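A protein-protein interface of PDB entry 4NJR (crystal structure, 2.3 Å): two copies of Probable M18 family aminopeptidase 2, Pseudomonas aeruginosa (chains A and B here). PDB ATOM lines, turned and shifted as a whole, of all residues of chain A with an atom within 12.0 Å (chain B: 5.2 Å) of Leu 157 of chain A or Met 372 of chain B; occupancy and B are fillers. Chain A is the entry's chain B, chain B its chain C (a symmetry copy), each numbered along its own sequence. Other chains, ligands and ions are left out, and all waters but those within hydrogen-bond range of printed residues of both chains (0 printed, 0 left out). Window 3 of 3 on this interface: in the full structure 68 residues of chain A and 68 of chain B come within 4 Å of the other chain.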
ATOM      1  N   ASN A  99     -17.815 -42.162 -15.829  1.00  0.00           N
ATOM      2  CA  ASN A  99     -18.125 -40.883 -16.463  1.00  0.00           C
ATOM      3  C   ASN A  99     -18.147 -40.962 -18.021  1.00  0.00           C
ATOM      4  O   ASN A  99     -17.663 -40.102 -18.685  1.00  0.00           O
ATOM      5  CB  ASN A  99     -17.096 -39.879 -16.041  1.00  0.00           C
ATOM      6  CG  ASN A  99     -16.962 -39.774 -14.535  1.00  0.00           C
ATOM      7  OD1 ASN A  99     -17.852 -39.304 -13.814  1.00  0.00           O
ATOM      8  ND2 ASN A  99     -15.841 -40.130 -14.071  1.00  0.00           N
ATOM      9  N   PRO A 151      -4.676 -37.818 -19.222  1.00  0.00           N
ATOM     10  CA  PRO A 151      -4.631 -36.375 -19.080  1.00  0.00           C
ATOM     11  C   PRO A 151      -4.275 -35.877 -17.671  1.00  0.00           C
ATOM     12  O   PRO A 151      -4.760 -36.442 -16.662  1.00  0.00           O
ATOM     13  CB  PRO A 151      -6.074 -35.949 -19.414  1.00  0.00           C
ATOM     14  CG  PRO A 151      -6.803 -37.186 -19.798  1.00  0.00           C
ATOM     15  CD  PRO A 151      -6.044 -38.330 -19.242  1.00  0.00           C
ATOM     16  N   ASN A 152      -3.510 -34.788 -17.598  1.00  0.00           N
ATOM     17  CA  ASN A 152      -3.392 -34.095 -16.313  1.00  0.00           C
ATOM     18  C   ASN A 152      -4.711 -33.564 -15.811  1.00  0.00           C
ATOM     19  O   ASN A 152      -5.622 -33.381 -16.581  1.00  0.00           O
ATOM     20  CB  ASN A 152      -2.376 -33.005 -16.342  1.00  0.00           C
ATOM     21  CG  ASN A 152      -1.004 -33.479 -15.862  1.00  0.00           C
ATOM     22  OD1 ASN A 152      -0.840 -33.957 -14.748  1.00  0.00           O
ATOM     23  ND2 ASN A 152      -0.027 -33.362 -16.713  1.00  0.00           N
ATOM     24  N   LEU A 153      -4.838 -33.426 -14.498  1.00  0.00           N
ATOM     25  CA  LEU A 153      -5.926 -32.635 -13.912  1.00  0.00           C
ATOM     26  C   LEU A 153      -5.574 -31.161 -14.099  1.00  0.00           C
ATOM     27  O   LEU A 153      -4.437 -30.792 -13.875  1.00  0.00           O
ATOM     28  CB  LEU A 153      -6.089 -32.944 -12.396  1.00  0.00           C
ATOM     29  CG  LEU A 153      -7.117 -32.090 -11.648  1.00  0.00           C
ATOM     30  CD1 LEU A 153      -8.535 -32.267 -12.218  1.00  0.00           C
ATOM     31  CD2 LEU A 153      -7.093 -32.469 -10.170  1.00  0.00           C
ATOM     32  N   ALA A 154      -6.523 -30.332 -14.512  1.00  0.00           N
ATOM     33  CA  ALA A 154      -6.266 -28.884 -14.700  1.00  0.00           C
ATOM     34  C   ALA A 154      -5.658 -28.251 -13.442  1.00  0.00           C
ATOM     35  O   ALA A 154      -6.060 -28.587 -12.328  1.00  0.00           O
ATOM     36  CB  ALA A 154      -7.580 -28.155 -14.988  1.00  0.00           C
ATOM     37  N   ILE A 155      -4.773 -27.288 -13.616  1.00  0.00           N
ATOM     38  CA  ILE A 155      -4.225 -26.582 -12.471  1.00  0.00           C
ATOM     39  C   ILE A 155      -5.298 -25.875 -11.637  1.00  0.00           C
ATOM     40  O   ILE A 155      -5.185 -25.837 -10.401  1.00  0.00           O
ATOM     41  CB  ILE A 155      -3.074 -25.631 -12.843  1.00  0.00           C
ATOM     42  CG1 ILE A 155      -2.318 -25.152 -11.605  1.00  0.00           C
ATOM     43  CG2 ILE A 155      -3.582 -24.420 -13.627  1.00  0.00           C
ATOM     44  CD1 ILE A 155      -0.996 -24.476 -11.943  1.00  0.00           C
ATOM     45  N   HIS A 156      -6.331 -25.352 -12.315  1.00  0.00           N
ATOM     46  CA  HIS A 156      -7.492 -24.736 -11.674  1.00  0.00           C
ATOM     47  C   HIS A 156      -8.122 -25.598 -10.622  1.00  0.00           C
ATOM     48  O   HIS A 156      -8.678 -25.053  -9.709  1.00  0.00           O
ATOM     49  CB  HIS A 156      -8.566 -24.387 -12.662  1.00  0.00           C
ATOM     50  CG  HIS A 156      -8.038 -23.691 -13.871  1.00  0.00           C
ATOM     51  ND1 HIS A 156      -7.278 -24.337 -14.833  1.00  0.00           N
ATOM     52  CD2 HIS A 156      -8.075 -22.387 -14.229  1.00  0.00           C
ATOM     53  CE1 HIS A 156      -6.894 -23.462 -15.741  1.00  0.00           C
ATOM     54  NE2 HIS A 156      -7.354 -22.273 -15.393  1.00  0.00           N
ATOM     55  N   LEU A 157      -8.026 -26.922 -10.716  1.00  0.00           N
ATOM     56  CA  LEU A 157      -8.653 -27.852  -9.752  1.00  0.00           C
ATOM     57  C   LEU A 157      -7.622 -28.569  -8.893  1.00  0.00           C
ATOM     58  O   LEU A 157      -7.932 -29.557  -8.237  1.00  0.00           O
ATOM     59  CB  LEU A 157      -9.410 -28.922 -10.536  1.00  0.00           C
ATOM     60  CG  LEU A 157     -10.507 -28.369 -11.474  1.00  0.00           C
ATOM     61  CD1 LEU A 157     -11.040 -29.407 -12.416  1.00  0.00           C
ATOM     62  CD2 LEU A 157     -11.662 -27.832 -10.634  1.00  0.00           C
ATOM     63  N   ASN A 158      -6.384 -28.097  -8.958  1.00  0.00           N
ATOM     64  CA  ASN A 158      -5.257 -28.710  -8.275  1.00  0.00           C
ATOM     65  C   ASN A 158      -4.239 -27.584  -8.181  1.00  0.00           C
ATOM     66  O   ASN A 158      -3.175 -27.668  -8.749  1.00  0.00           O
ATOM     67  CB  ASN A 158      -4.719 -29.893  -9.108  1.00  0.00           C
ATOM     68  CG  ASN A 158      -3.489 -30.537  -8.487  1.00  0.00           C
ATOM     69  OD1 ASN A 158      -3.195 -30.341  -7.325  1.00  0.00           O
ATOM     70  ND2 ASN A 158      -2.751 -31.272  -9.279  1.00  0.00           N
ATOM     71  N   ARG A 159      -4.628 -26.506  -7.515  1.00  0.00           N
ATOM     72  CA  ARG A 159      -3.900 -25.222  -7.481  1.00  0.00           C
ATOM     73  C   ARG A 159      -2.448 -25.324  -7.009  1.00  0.00           C
ATOM     74  O   ARG A 159      -1.608 -24.528  -7.429  1.00  0.00           O
ATOM     75  CB  ARG A 159      -4.612 -24.248  -6.530  1.00  0.00           C
ATOM     76  CG  ARG A 159      -5.902 -23.659  -7.046  1.00  0.00           C
ATOM     77  CD  ARG A 159      -5.625 -22.331  -7.712  1.00  0.00           C
ATOM     78  NE  ARG A 159      -6.815 -21.864  -8.420  1.00  0.00           N
ATOM     79  CZ  ARG A 159      -6.835 -21.285  -9.628  1.00  0.00           C
ATOM     80  NH1 ARG A 159      -5.709 -21.077 -10.329  1.00  0.00           N
ATOM     81  NH2 ARG A 159      -8.009 -20.926 -10.149  1.00  0.00           N
ATOM     82  N   ALA A 160      -2.152 -26.249  -6.107  1.00  0.00           N
ATOM     83  CA  ALA A 160      -0.765 -26.464  -5.690  1.00  0.00           C
ATOM     84  C   ALA A 160      -0.047 -27.596  -6.491  1.00  0.00           C
ATOM     85  O   ALA A 160       0.982 -28.093  -6.036  1.00  0.00           O
ATOM     86  CB  ALA A 160      -0.687 -26.689  -4.160  1.00  0.00           C
ATOM     87  N   ALA A 161      -0.572 -27.968  -7.668  1.00  0.00           N
ATOM     88  CA  ALA A 161       0.055 -28.914  -8.586  1.00  0.00           C
ATOM     89  C   ALA A 161       1.559 -28.825  -8.699  1.00  0.00           C
ATOM     90  O   ALA A 161       2.244 -29.864  -8.669  1.00  0.00           O
ATOM     91  CB  ALA A 161      -0.527 -28.778  -9.999  1.00  0.00           C
ATOM     92  N   ASN A 162       2.069 -27.599  -8.839  1.00  0.00           N
ATOM     93  CA  ASN A 162       3.522 -27.348  -8.962  1.00  0.00           C
ATOM     94  C   ASN A 162       4.302 -27.513  -7.639  1.00  0.00           C
ATOM     95  O   ASN A 162       5.521 -27.573  -7.651  1.00  0.00           O
ATOM     96  CB  ASN A 162       3.811 -25.963  -9.628  1.00  0.00           C
ATOM     97  CG  ASN A 162       3.291 -25.878 -11.077  1.00  0.00           C
ATOM     98  OD1 ASN A 162       3.296 -26.852 -11.820  1.00  0.00           O
ATOM     99  ND2 ASN A 162       2.808 -24.725 -11.456  1.00  0.00           N
ATOM    100  N   GLU A 163       3.606 -27.644  -6.519  1.00  0.00           N
ATOM    101  CA  GLU A 163       4.274 -27.967  -5.256  1.00  0.00           C
ATOM    102  C   GLU A 163       4.618 -29.440  -5.174  1.00  0.00           C
ATOM    103  O   GLU A 163       5.468 -29.795  -4.385  1.00  0.00           O
ATOM    104  CB  GLU A 163       3.414 -27.651  -4.052  1.00  0.00           C
ATOM    105  CG  GLU A 163       2.798 -26.269  -4.076  1.00  0.00           C
ATOM    106  CD  GLU A 163       3.699 -25.223  -3.486  1.00  0.00           C
ATOM    107  OE1 GLU A 163       3.155 -24.307  -2.812  1.00  0.00           O
ATOM    108  OE2 GLU A 163       4.935 -25.327  -3.677  1.00  0.00           O
ATOM    109  N   GLY A 164       4.022 -30.265  -6.038  1.00  0.00           N
ATOM    110  CA  GLY A 164       4.275 -31.699  -6.034  1.00  0.00           C
ATOM    111  C   GLY A 164       3.163 -32.373  -5.241  1.00  0.00           C
ATOM    112  O   GLY A 164       2.664 -31.777  -4.259  1.00  0.00           O
ATOM    113  N   TRP A 165       2.696 -33.530  -5.712  1.00  0.00           N
ATOM    114  CA  TRP A 165       1.893 -34.451  -4.896  1.00  0.00           C
ATOM    115  C   TRP A 165       2.319 -35.883  -5.267  1.00  0.00           C
ATOM    116  O   TRP A 165       2.903 -36.069  -6.327  1.00  0.00           O
ATOM    117  CB  TRP A 165       0.388 -34.254  -5.142  1.00  0.00           C
ATOM    118  CG  TRP A 165      -0.065 -34.776  -6.473  1.00  0.00           C
ATOM    119  CD1 TRP A 165      -0.675 -35.975  -6.692  1.00  0.00           C
ATOM    120  CD2 TRP A 165       0.082 -34.147  -7.770  1.00  0.00           C
ATOM    121  NE1 TRP A 165      -0.951 -36.119  -8.030  1.00  0.00           N
ATOM    122  CE2 TRP A 165      -0.492 -35.024  -8.721  1.00  0.00           C
ATOM    123  CE3 TRP A 165       0.623 -32.926  -8.215  1.00  0.00           C
ATOM    124  CZ2 TRP A 165      -0.528 -34.737 -10.132  1.00  0.00           C
ATOM    125  CZ3 TRP A 165       0.581 -32.625  -9.626  1.00  0.00           C
ATOM    126  CH2 TRP A 165       0.010 -33.552 -10.559  1.00  0.00           C
ATOM    127  N   GLU A 172      -4.469 -42.600 -10.942  1.00  0.00           N
ATOM    128  CA  GLU A 172      -4.213 -41.457 -11.819  1.00  0.00           C
ATOM    129  C   GLU A 172      -3.645 -41.867 -13.171  1.00  0.00           C
ATOM    130  O   GLU A 172      -3.592 -41.063 -14.064  1.00  0.00           O
ATOM    131  CB  GLU A 172      -3.245 -40.489 -11.123  1.00  0.00           C
ATOM    132  CG  GLU A 172      -3.882 -39.785  -9.893  1.00  0.00           C
ATOM    133  CD  GLU A 172      -2.914 -38.892  -9.159  1.00  0.00           C
ATOM    134  OE1 GLU A 172      -2.443 -37.923  -9.782  1.00  0.00           O
ATOM    135  OE2 GLU A 172      -2.581 -39.210  -8.007  1.00  0.00           O
ATOM    136  N   HIS B 310     -13.944 -27.091 -17.655  1.00  0.00           N
ATOM    137  CA  HIS B 310     -13.398 -28.342 -17.127  1.00  0.00           C
ATOM    138  C   HIS B 310     -14.391 -29.461 -17.254  1.00  0.00           C
ATOM    139  O   HIS B 310     -15.444 -29.497 -16.590  1.00  0.00           O
ATOM    140  CB  HIS B 310     -13.093 -28.202 -15.634  1.00  0.00           C
ATOM    141  CG  HIS B 310     -12.154 -27.111 -15.344  1.00  0.00           C
ATOM    142  ND1 HIS B 310     -10.853 -27.127 -15.786  1.00  0.00           N
ATOM    143  CD2 HIS B 310     -12.328 -25.929 -14.707  1.00  0.00           C
ATOM    144  CE1 HIS B 310     -10.249 -26.009 -15.407  1.00  0.00           C
ATOM    145  NE2 HIS B 310     -11.116 -25.276 -14.732  1.00  0.00           N
ATOM    146  N   ARG B 319     -13.132 -33.969  -8.116  1.00  0.00           N
ATOM    147  CA  ARG B 319     -12.865 -32.517  -8.262  1.00  0.00           C
ATOM    148  C   ARG B 319     -14.046 -31.752  -8.828  1.00  0.00           C
ATOM    149  O   ARG B 319     -14.052 -30.558  -8.845  1.00  0.00           O
ATOM    150  CB  ARG B 319     -11.629 -32.264  -9.105  1.00  0.00           C
ATOM    151  CG  ARG B 319     -10.419 -32.891  -8.473  1.00  0.00           C
ATOM    152  CD  ARG B 319      -9.817 -32.147  -7.303  1.00  0.00           C
ATOM    153  NE  ARG B 319      -8.713 -32.962  -6.749  1.00  0.00           N
ATOM    154  CZ  ARG B 319      -7.537 -32.523  -6.270  1.00  0.00           C
ATOM    155  NH1 ARG B 319      -7.201 -31.225  -6.215  1.00  0.00           N
ATOM    156  NH2 ARG B 319      -6.687 -33.417  -5.804  1.00  0.00           N
ATOM    157  N   HIS B 320     -15.031 -32.469  -9.288  1.00  0.00           N
ATOM    158  CA  HIS B 320     -16.278 -31.886  -9.765  1.00  0.00           C
ATOM    159  C   HIS B 320     -17.427 -32.122  -8.798  1.00  0.00           C
ATOM    160  O   HIS B 320     -17.447 -33.092  -8.055  1.00  0.00           O
ATOM    161  CB  HIS B 320     -16.638 -32.489 -11.123  1.00  0.00           C
ATOM    162  CG  HIS B 320     -16.003 -31.765 -12.247  1.00  0.00           C
ATOM    163  ND1 HIS B 320     -14.643 -31.844 -12.503  1.00  0.00           N
ATOM    164  CD2 HIS B 320     -16.520 -30.911 -13.163  1.00  0.00           C
ATOM    165  CE1 HIS B 320     -14.360 -31.080 -13.539  1.00  0.00           C
ATOM    166  NE2 HIS B 320     -15.481 -30.504 -13.952  1.00  0.00           N
ATOM    167  N   THR B 368     -18.671 -24.924  -9.936  1.00  0.00           N
ATOM    168  CA  THR B 368     -17.608 -25.507  -9.068  1.00  0.00           C
ATOM    169  C   THR B 368     -18.173 -26.252  -7.815  1.00  0.00           C
ATOM    170  O   THR B 368     -19.240 -25.909  -7.249  1.00  0.00           O
ATOM    171  CB  THR B 368     -16.625 -24.388  -8.605  1.00  0.00           C
ATOM    172  OG1 THR B 368     -15.579 -24.955  -7.841  1.00  0.00           O
ATOM    173  CG2 THR B 368     -17.284 -23.427  -7.689  1.00  0.00           C
ATOM    174  N   ARG B 369     -17.457 -27.248  -7.334  1.00  0.00           N
ATOM    175  CA  ARG B 369     -17.724 -27.701  -5.951  1.00  0.00           C
ATOM    176  C   ARG B 369     -17.787 -26.508  -5.009  1.00  0.00           C
ATOM    177  O   ARG B 369     -16.985 -25.568  -5.110  1.00  0.00           O
ATOM    178  CB  ARG B 369     -16.658 -28.627  -5.455  1.00  0.00           C
ATOM    179  CG  ARG B 369     -16.662 -30.001  -6.072  1.00  0.00           C
ATOM    180  CD  ARG B 369     -15.500 -30.818  -5.471  1.00  0.00           C
ATOM    181  NE  ARG B 369     -15.531 -30.807  -3.987  1.00  0.00           N
ATOM    182  CZ  ARG B 369     -15.825 -31.855  -3.216  1.00  0.00           C
ATOM    183  NH1 ARG B 369     -16.102 -33.028  -3.763  1.00  0.00           N
ATOM    184  NH2 ARG B 369     -15.838 -31.741  -1.876  1.00  0.00           N
ATOM    185  N   SER B 370     -18.746 -26.513  -4.096  1.00  0.00           N
ATOM    186  CA  SER B 370     -18.935 -25.328  -3.247  1.00  0.00           C
ATOM    187  C   SER B 370     -17.807 -25.123  -2.198  1.00  0.00           C
ATOM    188  O   SER B 370     -17.699 -24.054  -1.619  1.00  0.00           O
ATOM    189  CB  SER B 370     -20.317 -25.337  -2.616  1.00  0.00           C
ATOM    190  OG  SER B 370     -21.304 -25.355  -3.632  1.00  0.00           O
ATOM    191  N   ASP B 371     -16.908 -26.093  -2.053  1.00  0.00           N
ATOM    192  CA  ASP B 371     -15.739 -25.962  -1.179  1.00  0.00           C
ATOM    193  C   ASP B 371     -14.458 -25.652  -1.937  1.00  0.00           C
ATOM    194  O   ASP B 371     -13.387 -25.761  -1.363  1.00  0.00           O
ATOM    195  CB  ASP B 371     -15.533 -27.236  -0.331  1.00  0.00           C
ATOM    196  CG  ASP B 371     -15.348 -28.513  -1.173  1.00  0.00           C
ATOM    197  OD1 ASP B 371     -15.411 -28.496  -2.414  1.00  0.00           O
ATOM    198  OD2 ASP B 371     -15.137 -29.570  -0.572  1.00  0.00           O
ATOM    199  N   MET B 372     -14.570 -25.313  -3.213  1.00  0.00           N
ATOM    200  CA  MET B 372     -13.426 -24.915  -4.045  1.00  0.00           C
ATOM    201  C   MET B 372     -13.753 -23.582  -4.720  1.00  0.00           C
ATOM    202  O   MET B 372     -14.888 -23.368  -5.173  1.00  0.00           O
ATOM    203  CB  MET B 372     -13.161 -25.942  -5.179  1.00  0.00           C
ATOM    204  CG  MET B 372     -12.696 -27.347  -4.748  1.00  0.00           C
ATOM    205  SD  MET B 372     -12.359 -28.547  -6.095  1.00  0.00           S
ATOM    206  CE  MET B 372     -10.632 -28.194  -6.418  1.00  0.00           C
ATOM    207  N   GLY B 373     -12.751 -22.711  -4.819  1.00  0.00           N
ATOM    208  CA  GLY B 373     -12.790 -21.609  -5.781  1.00  0.00           C
ATOM    209  C   GLY B 373     -13.002 -22.147  -7.192  1.00  0.00           C
ATOM    210  O   GLY B 373     -13.325 -21.394  -8.116  1.00  0.00           O
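The backbone carbonyl oxygen (O) of Leu 157 of chain A sits at hydrogen-bond distance from the guanidinium group (NH1) of Arg 319 of chain B (2.7 Å).
Printed residues of chain B that touch a printed residue of chain A: His 310, Arg 319, His 320 and Met 372. Hydrophobic or aromatic side chains of chain A within 4 Å of the printed part of chain B: Leu 153, Ala 154, His 156 and Leu 157. Among the printed residues, 8 pairs touch across the chains.
Of the printed residues of chain B, Leu 153 of chain A touches Arg 319 (3.8 Å). Of the printed residues of chain B, Ala 154 of chain A touches His 310 (3.5 Å). Of the printed residues of chain B, His 156 of chain A touches His 310 (3.4 Å). Leu 157 of chain A touches four residues of chain B. Of the printed residues of chain B, Asn 158 of chain A touches Arg 319. Ala 160 of chain A touches none of the printed residues of chain B. Gly 164 of chain A touches none of the printed residues of chain B. Of chain A, only Leu 153 (3.8 Å), Leu 157 (2.7 Å) and Asn 158 (3.8 Å) come within 4 Å of Arg 319 of chain B. His 320 of chain B touches just one residue of chain A: Leu 157 (3.9 Å). No residue of chain A comes within 4 Å of Thr 368 of chain B. No residue of chain A comes within 4 Å of Asp 371 of chain B. Met 372 of chain B touches one residue of chain A. Gly 373 of chain B touches none of the printed residues of chain A. The nearest printed residue of chain B that does not touch Leu 157 of chain A is Thr 368 of chain B (5.6 Å).
O of His 310 of chain B is in hydrogen-bond range of NE2 of His 320 of chain B. The side-chain hydroxyl (OG1) of Thr 368 of chain B lies within hydrogen-bond range of the backbone carbonyl oxygen (O) of Met 372 of chain B (3.2 Å).
Among the printed residues, merely in contact across the chains: His 156 of chain A with His 310 of chain B, Ala 154 of chain A with His 310 of chain B, Leu 157 of chain A with Met 372 of chain B, Leu 153 of chain A with Arg 319 of chain B, Asn 158 of chain A with Arg 319 of chain B, Leu 157 of chain A with His 320 of chain B and Leu 157 of chain A with His 310 of chain B.
No position is printed for both chains.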
